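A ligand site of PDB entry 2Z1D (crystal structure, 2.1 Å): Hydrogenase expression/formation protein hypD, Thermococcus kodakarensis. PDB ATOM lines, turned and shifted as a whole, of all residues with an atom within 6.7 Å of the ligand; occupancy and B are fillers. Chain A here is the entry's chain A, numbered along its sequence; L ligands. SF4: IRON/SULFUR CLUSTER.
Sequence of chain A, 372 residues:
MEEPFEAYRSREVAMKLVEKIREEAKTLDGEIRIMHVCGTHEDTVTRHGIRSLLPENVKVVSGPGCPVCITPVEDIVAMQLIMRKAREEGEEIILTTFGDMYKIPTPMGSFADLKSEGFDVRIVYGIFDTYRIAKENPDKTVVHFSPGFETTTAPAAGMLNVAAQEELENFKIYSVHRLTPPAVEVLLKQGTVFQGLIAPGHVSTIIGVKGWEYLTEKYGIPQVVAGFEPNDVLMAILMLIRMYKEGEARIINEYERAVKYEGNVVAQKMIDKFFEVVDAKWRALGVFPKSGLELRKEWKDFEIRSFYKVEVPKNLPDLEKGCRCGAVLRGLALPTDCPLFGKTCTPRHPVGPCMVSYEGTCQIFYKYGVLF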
ATOM      1  N   LEU A 319      20.564  13.624  -7.707  1.00  0.00           N
ATOM      2  CA  LEU A 319      21.360  14.044  -8.867  1.00  0.00           C
ATOM      3  C   LEU A 319      21.357  15.540  -9.135  1.00  0.00           C
ATOM      4  O   LEU A 319      20.454  16.259  -8.723  1.00  0.00           O
ATOM      5  CB  LEU A 319      20.840  13.328 -10.131  1.00  0.00           C
ATOM      6  CG  LEU A 319      20.720  11.804 -10.085  1.00  0.00           C
ATOM      7  CD1 LEU A 319      19.959  11.284 -11.331  1.00  0.00           C
ATOM      8  CD2 LEU A 319      22.109  11.202  -9.970  1.00  0.00           C
ATOM      9  N   GLU A 320      22.378  16.004  -9.847  1.00  0.00           N
ATOM     10  CA  GLU A 320      22.463  17.408 -10.214  1.00  0.00           C
ATOM     11  C   GLU A 320      21.467  17.638 -11.354  1.00  0.00           C
ATOM     12  O   GLU A 320      21.094  16.696 -12.053  1.00  0.00           O
ATOM     13  CB  GLU A 320      23.878  17.762 -10.684  1.00  0.00           C
ATOM     14  CG  GLU A 320      24.910  17.790  -9.551  1.00  0.00           C
ATOM     15  CD  GLU A 320      26.312  18.176 -10.015  1.00  0.00           C
ATOM     16  OE1 GLU A 320      26.430  19.152 -10.790  1.00  0.00           O
ATOM     17  OE2 GLU A 320      27.301  17.509  -9.593  1.00  0.00           O
ATOM     18  N   LYS A 321      21.074  18.882 -11.551  1.00  0.00           N
ATOM     19  CA  LYS A 321      20.093  19.254 -12.580  1.00  0.00           C
ATOM     20  C   LYS A 321      20.325  18.707 -13.986  1.00  0.00           C
ATOM     21  O   LYS A 321      21.365  18.958 -14.599  1.00  0.00           O
ATOM     22  CB  LYS A 321      19.965  20.783 -12.642  1.00  0.00           C
ATOM     23  CG  LYS A 321      18.888  21.300 -13.579  1.00  0.00           C
ATOM     24  CD  LYS A 321      18.694  22.804 -13.391  1.00  0.00           C
ATOM     25  CE  LYS A 321      17.578  23.353 -14.275  1.00  0.00           C
ATOM     26  NZ  LYS A 321      17.233  24.762 -13.897  1.00  0.00           N
ATOM     27  N   GLY A 322      19.346  17.980 -14.509  1.00  0.00           N
ATOM     28  CA  GLY A 322      19.481  17.457 -15.856  1.00  0.00           C
ATOM     29  C   GLY A 322      20.158  16.107 -16.010  1.00  0.00           C
ATOM     30  O   GLY A 322      20.129  15.527 -17.091  1.00  0.00           O
ATOM     31  N   CYS A 323      20.784  15.594 -14.948  1.00  0.00           N
ATOM     32  CA  CYS A 323      21.444  14.280 -15.041  1.00  0.00           C
ATOM     33  C   CYS A 323      20.407  13.172 -15.267  1.00  0.00           C
ATOM     34  O   CYS A 323      19.454  13.046 -14.509  1.00  0.00           O
ATOM     35  CB  CYS A 323      22.224  13.977 -13.753  1.00  0.00           C
ATOM     36  SG  CYS A 323      22.977  12.318 -13.699  1.00  0.00           S
ATOM     37  N   ARG A 324      20.600  12.358 -16.317  1.00  0.00           N
ATOM     38  CA  ARG A 324      19.676  11.261 -16.624  1.00  0.00           C
ATOM     39  C   ARG A 324      20.194   9.904 -16.126  1.00  0.00           C
ATOM     40  O   ARG A 324      19.767   8.838 -16.587  1.00  0.00           O
ATOM     41  CB  ARG A 324      19.428  11.187 -18.133  1.00  0.00           C
ATOM     42  CG  ARG A 324      19.019  12.508 -18.810  1.00  0.00           C
ATOM     43  CD  ARG A 324      17.673  13.011 -18.336  1.00  0.00           C
ATOM     44  NE  ARG A 324      16.979  13.808 -19.351  1.00  0.00           N
ATOM     45  CZ  ARG A 324      17.128  15.119 -19.536  1.00  0.00           C
ATOM     46  NH1 ARG A 324      17.967  15.836 -18.772  1.00  0.00           N
ATOM     47  NH2 ARG A 324      16.419  15.733 -20.476  1.00  0.00           N
ATOM     48  N   CYS A 325      21.143   9.943 -15.190  1.00  0.00           N
ATOM     49  CA  CYS A 325      21.729   8.737 -14.645  1.00  0.00           C
ATOM     50  C   CYS A 325      20.644   7.779 -14.134  1.00  0.00           C
ATOM     51  O   CYS A 325      20.850   6.565 -14.085  1.00  0.00           O
ATOM     52  CB  CYS A 325      22.740   9.106 -13.549  1.00  0.00           C
ATOM     53  SG  CYS A 325      23.849   7.788 -12.905  1.00  0.00           S
ATOM     54  N   GLY A 326      19.465   8.301 -13.765  1.00  0.00           N
ATOM     55  CA  GLY A 326      18.377   7.444 -13.343  1.00  0.00           C
ATOM     56  C   GLY A 326      17.881   6.557 -14.482  1.00  0.00           C
ATOM     57  O   GLY A 326      17.686   5.343 -14.312  1.00  0.00           O
ATOM     58  N   VAL A 328      19.519   5.969 -17.302  1.00  0.00           N
ATOM     59  CA  VAL A 328      20.666   5.162 -17.716  1.00  0.00           C
ATOM     60  C   VAL A 328      20.846   3.920 -16.852  1.00  0.00           C
ATOM     61  O   VAL A 328      21.083   2.823 -17.377  1.00  0.00           O
ATOM     62  CB  VAL A 328      21.950   5.997 -17.691  1.00  0.00           C
ATOM     63  CG1 VAL A 328      23.149   5.126 -18.028  1.00  0.00           C
ATOM     64  CG2 VAL A 328      21.824   7.145 -18.683  1.00  0.00           C
ATOM     65  N   LEU A 334      20.644   5.567 -23.013  1.00  0.00           N
ATOM     66  CA  LEU A 334      22.080   5.401 -23.109  1.00  0.00           C
ATOM     67  C   LEU A 334      22.665   6.777 -22.806  1.00  0.00           C
ATOM     68  O   LEU A 334      21.964   7.791 -22.909  1.00  0.00           O
ATOM     69  CB  LEU A 334      22.457   4.914 -24.507  1.00  0.00           C
ATOM     70  CG  LEU A 334      21.939   3.492 -24.766  1.00  0.00           C
ATOM     71  CD1 LEU A 334      22.237   3.083 -26.201  1.00  0.00           C
ATOM     72  CD2 LEU A 334      22.582   2.512 -23.788  1.00  0.00           C
ATOM     73  N   PRO A 335      23.940   6.839 -22.409  1.00  0.00           N
ATOM     74  CA  PRO A 335      24.495   8.165 -22.114  1.00  0.00           C
ATOM     75  C   PRO A 335      24.336   9.155 -23.266  1.00  0.00           C
ATOM     76  O   PRO A 335      24.201  10.340 -23.026  1.00  0.00           O
ATOM     77  CB  PRO A 335      25.962   7.891 -21.761  1.00  0.00           C
ATOM     78  CG  PRO A 335      26.165   6.426 -21.977  1.00  0.00           C
ATOM     79  CD  PRO A 335      24.829   5.770 -21.939  1.00  0.00           C
ATOM     80  N   CYS A 338      21.566  11.517 -23.004  1.00  0.00           N
ATOM     81  CA  CYS A 338      21.609  12.566 -22.005  1.00  0.00           C
ATOM     82  C   CYS A 338      22.125  13.877 -22.599  1.00  0.00           C
ATOM     83  O   CYS A 338      23.214  13.940 -23.143  1.00  0.00           O
ATOM     84  CB  CYS A 338      22.490  12.162 -20.825  1.00  0.00           C
ATOM     85  SG  CYS A 338      22.699  13.554 -19.688  1.00  0.00           S
ATOM     86  N   PRO A 339      21.334  14.959 -22.464  1.00  0.00           N
ATOM     87  CA  PRO A 339      21.739  16.261 -22.999  1.00  0.00           C
ATOM     88  C   PRO A 339      22.999  16.885 -22.401  1.00  0.00           C
ATOM     89  O   PRO A 339      23.526  17.849 -22.926  1.00  0.00           O
ATOM     90  CB  PRO A 339      20.486  17.123 -22.793  1.00  0.00           C
ATOM     91  CG  PRO A 339      19.888  16.518 -21.541  1.00  0.00           C
ATOM     92  CD  PRO A 339      20.039  15.040 -21.764  1.00  0.00           C
ATOM     93  N   LEU A 340      23.477  16.334 -21.284  1.00  0.00           N
ATOM     94  CA  LEU A 340      24.689  16.873 -20.670  1.00  0.00           C
ATOM     95  C   LEU A 340      25.950  16.091 -21.091  1.00  0.00           C
ATOM     96  O   LEU A 340      27.072  16.584 -20.969  1.00  0.00           O
ATOM     97  CB  LEU A 340      24.552  16.864 -19.138  1.00  0.00           C
ATOM     98  CG  LEU A 340      23.327  17.588 -18.568  1.00  0.00           C
ATOM     99  CD1 LEU A 340      23.404  17.596 -17.050  1.00  0.00           C
ATOM    100  CD2 LEU A 340      23.270  19.032 -19.111  1.00  0.00           C
ATOM    101  N   PHE A 341      25.735  14.880 -21.607  1.00  0.00           N
ATOM    102  CA  PHE A 341      26.824  13.999 -22.022  1.00  0.00           C
ATOM    103  C   PHE A 341      27.845  14.644 -22.959  1.00  0.00           C
ATOM    104  O   PHE A 341      27.540  14.970 -24.107  1.00  0.00           O
ATOM    105  CB  PHE A 341      26.237  12.753 -22.699  1.00  0.00           C
ATOM    106  CG  PHE A 341      27.276  11.736 -23.112  1.00  0.00           C
ATOM    107  CD1 PHE A 341      27.972  11.000 -22.161  1.00  0.00           C
ATOM    108  CD2 PHE A 341      27.579  11.530 -24.455  1.00  0.00           C
ATOM    109  CE1 PHE A 341      28.975  10.083 -22.538  1.00  0.00           C
ATOM    110  CE2 PHE A 341      28.571  10.624 -24.849  1.00  0.00           C
ATOM    111  CZ  PHE A 341      29.277   9.902 -23.883  1.00  0.00           C
ATOM    112  N   GLY A 342      29.062  14.816 -22.457  1.00  0.00           N
ATOM    113  CA  GLY A 342      30.118  15.410 -23.255  1.00  0.00           C
ATOM    114  C   GLY A 342      30.062  16.917 -23.354  1.00  0.00           C
ATOM    115  O   GLY A 342      30.921  17.537 -23.980  1.00  0.00           O
ATOM    116  N   THR A 344      28.335  19.533 -20.479  1.00  0.00           N
ATOM    117  CA  THR A 344      28.639  19.958 -19.135  1.00  0.00           C
ATOM    118  C   THR A 344      29.174  18.807 -18.300  1.00  0.00           C
ATOM    119  O   THR A 344      29.848  19.019 -17.304  1.00  0.00           O
ATOM    120  CB  THR A 344      27.410  20.607 -18.440  1.00  0.00           C
ATOM    121  OG1 THR A 344      26.279  19.722 -18.492  1.00  0.00           O
ATOM    122  CG2 THR A 344      27.047  21.924 -19.138  1.00  0.00           C
ATOM    123  N   CYS A 345      28.891  17.569 -18.719  1.00  0.00           N
ATOM    124  CA  CYS A 345      29.358  16.409 -17.971  1.00  0.00           C
ATOM    125  C   CYS A 345      30.433  15.607 -18.713  1.00  0.00           C
ATOM    126  O   CYS A 345      30.188  15.066 -19.795  1.00  0.00           O
ATOM    127  CB  CYS A 345      28.189  15.492 -17.629  1.00  0.00           C
ATOM    128  SG  CYS A 345      28.622  14.007 -16.645  1.00  0.00           S
ATOM    129  N   THR A 346      31.616  15.534 -18.128  1.00  0.00           N
ATOM    130  CA  THR A 346      32.724  14.769 -18.701  1.00  0.00           C
ATOM    131  C   THR A 346      33.540  14.215 -17.551  1.00  0.00           C
ATOM    132  O   THR A 346      33.288  14.549 -16.391  1.00  0.00           O
ATOM    133  CB  THR A 346      33.656  15.639 -19.583  1.00  0.00           C
ATOM    134  OG1 THR A 346      34.352  16.564 -18.746  1.00  0.00           O
ATOM    135  CG2 THR A 346      32.857  16.401 -20.616  1.00  0.00           C
ATOM    136  N   PRO A 350      32.582  16.037 -14.053  1.00  0.00           N
ATOM    137  CA  PRO A 350      31.369  15.223 -14.010  1.00  0.00           C
ATOM    138  C   PRO A 350      30.186  15.858 -13.301  1.00  0.00           C
ATOM    139  O   PRO A 350      30.336  16.510 -12.266  1.00  0.00           O
ATOM    140  CB  PRO A 350      31.830  13.962 -13.289  1.00  0.00           C
ATOM    141  CG  PRO A 350      32.851  14.506 -12.332  1.00  0.00           C
ATOM    142  CD  PRO A 350      33.629  15.466 -13.195  1.00  0.00           C
ATOM    143  N   VAL A 351      29.005  15.678 -13.874  1.00  0.00           N
ATOM    144  CA  VAL A 351      27.798  16.223 -13.283  1.00  0.00           C
ATOM    145  C   VAL A 351      27.179  15.111 -12.453  1.00  0.00           C
ATOM    146  O   VAL A 351      26.818  15.341 -11.294  1.00  0.00           O
ATOM    147  CB  VAL A 351      26.804  16.696 -14.382  1.00  0.00           C
ATOM    148  CG1 VAL A 351      25.442  17.037 -13.770  1.00  0.00           C
ATOM    149  CG2 VAL A 351      27.381  17.924 -15.064  1.00  0.00           C
ATOM    150  N   GLY A 352      27.096  13.905 -13.026  1.00  0.00           N
ATOM    151  CA  GLY A 352      26.508  12.777 -12.330  1.00  0.00           C
ATOM    152  C   GLY A 352      27.473  11.651 -11.978  1.00  0.00           C
ATOM    153  O   GLY A 352      28.618  11.645 -12.458  1.00  0.00           O
ATOM    154  N   PRO A 353      27.036  10.701 -11.142  1.00  0.00           N
ATOM    155  CA  PRO A 353      27.884   9.578 -10.731  1.00  0.00           C
ATOM    156  C   PRO A 353      28.180   8.608 -11.873  1.00  0.00           C
ATOM    157  O   PRO A 353      29.212   7.953 -11.890  1.00  0.00           O
ATOM    158  CB  PRO A 353      27.089   8.939  -9.597  1.00  0.00           C
ATOM    159  CG  PRO A 353      25.679   9.168 -10.024  1.00  0.00           C
ATOM    160  CD  PRO A 353      25.697  10.581 -10.550  1.00  0.00           C
ATOM    161  N   CYS A 354      27.250   8.515 -12.821  1.00  0.00           N
ATOM    162  CA  CYS A 354      27.390   7.636 -13.986  1.00  0.00           C
ATOM    163  C   CYS A 354      28.683   7.918 -14.780  1.00  0.00           C
ATOM    164  O   CYS A 354      29.210   7.034 -15.449  1.00  0.00           O
ATOM    165  CB  CYS A 354      26.187   7.812 -14.933  1.00  0.00           C
ATOM    166  SG  CYS A 354      24.643   6.874 -14.557  1.00  0.00           S
ATOM    167  N   MET A 355      29.199   9.140 -14.678  1.00  0.00           N
ATOM    168  CA  MET A 355      30.406   9.526 -15.433  1.00  0.00           C
ATOM    169  C   MET A 355      31.736   9.408 -14.685  1.00  0.00           C
ATOM    170  O   MET A 355      32.812   9.393 -15.293  1.00  0.00           O
ATOM    171  CB  MET A 355      30.256  10.956 -15.932  1.00  0.00           C
ATOM    172  CG  MET A 355      31.448  11.489 -16.736  1.00  0.00           C
ATOM    173  SD  MET A 355      31.607  10.691 -18.353  1.00  0.00           S
ATOM    174  CE  MET A 355      30.453  11.662 -19.329  1.00  0.00           C
ATOM    175  N   VAL A 356      31.652   9.340 -13.360  1.00  0.00           N
ATOM    176  CA  VAL A 356      32.818   9.262 -12.489  1.00  0.00           C
ATOM    177  C   VAL A 356      33.267   7.835 -12.231  1.00  0.00           C
ATOM    178  O   VAL A 356      34.468   7.528 -12.200  1.00  0.00           O
ATOM    179  CB  VAL A 356      32.495   9.920 -11.113  1.00  0.00           C
ATOM    180  CG1 VAL A 356      33.614   9.678 -10.115  1.00  0.00           C
ATOM    181  CG2 VAL A 356      32.263  11.395 -11.299  1.00  0.00           C
ATOM    182  N   THR A 361      28.352   3.517 -17.013  1.00  0.00           N
ATOM    183  CA  THR A 361      28.002   3.461 -18.414  1.00  0.00           C
ATOM    184  C   THR A 361      28.414   4.728 -19.167  1.00  0.00           C
ATOM    185  O   THR A 361      28.945   4.642 -20.269  1.00  0.00           O
ATOM    186  CB  THR A 361      26.505   3.195 -18.583  1.00  0.00           C
ATOM    187  OG1 THR A 361      26.175   1.978 -17.891  1.00  0.00           O
ATOM    188  CG2 THR A 361      26.124   3.051 -20.067  1.00  0.00           C
ATOM    189  N   CYS A 362      28.186   5.892 -18.559  1.00  0.00           N
ATOM    190  CA  CYS A 362      28.565   7.158 -19.188  1.00  0.00           C
ATOM    191  C   CYS A 362      30.092   7.299 -19.305  1.00  0.00           C
ATOM    192  O   CYS A 362      30.579   7.796 -20.315  1.00  0.00           O
ATOM    193  CB  CYS A 362      27.964   8.336 -18.389  1.00  0.00           C
ATOM    194  SG  CYS A 362      26.141   8.293 -18.237  1.00  0.00           S
ATOM    195  N   GLN A 363      30.845   6.862 -18.297  1.00  0.00           N
ATOM    196  CA  GLN A 363      32.303   6.944 -18.362  1.00  0.00           C
ATOM    197  C   GLN A 363      32.769   5.963 -19.443  1.00  0.00           C
ATOM    198  O   GLN A 363      33.692   6.251 -20.212  1.00  0.00           O
ATOM    199  CB  GLN A 363      32.941   6.557 -17.022  1.00  0.00           C
ATOM    200  CG  GLN A 363      34.479   6.616 -17.007  1.00  0.00           C
ATOM    201  CD  GLN A 363      35.143   5.430 -17.705  1.00  0.00           C
ATOM    202  OE1 GLN A 363      36.051   5.613 -18.511  1.00  0.00           O
ATOM    203  NE2 GLN A 363      34.695   4.219 -17.391  1.00  0.00           N
HETATM  204 FE1  SF4 L   1      25.607  10.360 -17.489  1.00  0.00          FE
HETATM  205 FE2  SF4 L   1      24.235  12.607 -18.204  1.00  0.00          FE
HETATM  206 FE3  SF4 L   1      24.372  11.929 -15.530  1.00  0.00          FE
HETATM  207 FE4  SF4 L   1      26.629  12.859 -16.784  1.00  0.00          FE
HETATM  208  S1  SF4 L   1      24.771  13.990 -16.512  1.00  0.00           S
HETATM  209  S2  SF4 L   1      26.487  10.971 -15.458  1.00  0.00           S
HETATM  210  S3  SF4 L   1      26.259  12.008 -18.929  1.00  0.00           S
HETATM  211  S4  SF4 L   1      23.351  10.802 -17.315  1.00  0.00           S
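The backbone NH (N) of Val 351 sits close to the side-chain sulfur (SG) of Cys 345 (3.3 Å).
O of Cys 354 lies within hydrogen-bond range of N of Gln 363 (3.3 Å).
The backbone NH of Cys 345 sits at hydrogen-bond distance from the backbone carbonyl oxygen of Leu 340 (3.1 Å).
The side-chain sulfur of Cys 338 sits close to the backbone NH of Leu 340.
The side-chain sulfur (SG) of Cys 354 forms a disulfide with the side-chain sulfur (SG) of Cys 325 (2.0 Å).
The backbone NH (N) of Cys 362 lies close to the backbone carbonyl oxygen (O) of Cys 354, 3.5 Å away.
The guanidinium group (NH1) of Arg 324 is in hydrogen-bond range of the backbone carbonyl oxygen (O) of Gly 322, at 2.8 Å.
N of Cys 325 lies close to SG of Cys 323 (3.4 Å).
S2 of the ligand sits close to O of Gly 352, 3.7 Å away.
Merely in contact with the ligand: Phe 341 (3.7 Å), Leu 340 (3.9 Å) and Val 351 (3.999 Å).
Hydrophobic or aromatic side chains within 4 Å of the ligand: Leu 340, Phe 341, Val 351 and Met 355.
Within 4 Å of the ligand: Cys 323, Arg 324, Cys 325, Cys 338, Leu 340, Phe 341, Cys 345, Val 351, Gly 352, Cys 354, Met 355 and Cys 362.
N of Arg 324 sits close to S4 of the ligand (3.3 Å).
An iron atom (FE2) of the ligand is bound by the side-chain sulfur of Cys 338, 2.3 Å away.
A sulfur (S2) of the ligand sits close to the backbone NH (N) of Met 355 (3.4 Å).
The side-chain sulfur (SG) of Cys 323 is bound to an iron atom (FE3) of the ligand.
The side-chain sulfur of Cys 362 is bound to an iron atom (FE1) of the ligand (2.3 Å).
S2 of the ligand lies close to N of Cys 354, at 3.7 Å.
A sulfur (S4) of the ligand lies close to the backbone NH (N) of Cys 325 (3.2 Å).
The side-chain sulfur (SG) of Cys 345 is bound to an iron atom (FE4) of the ligand.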
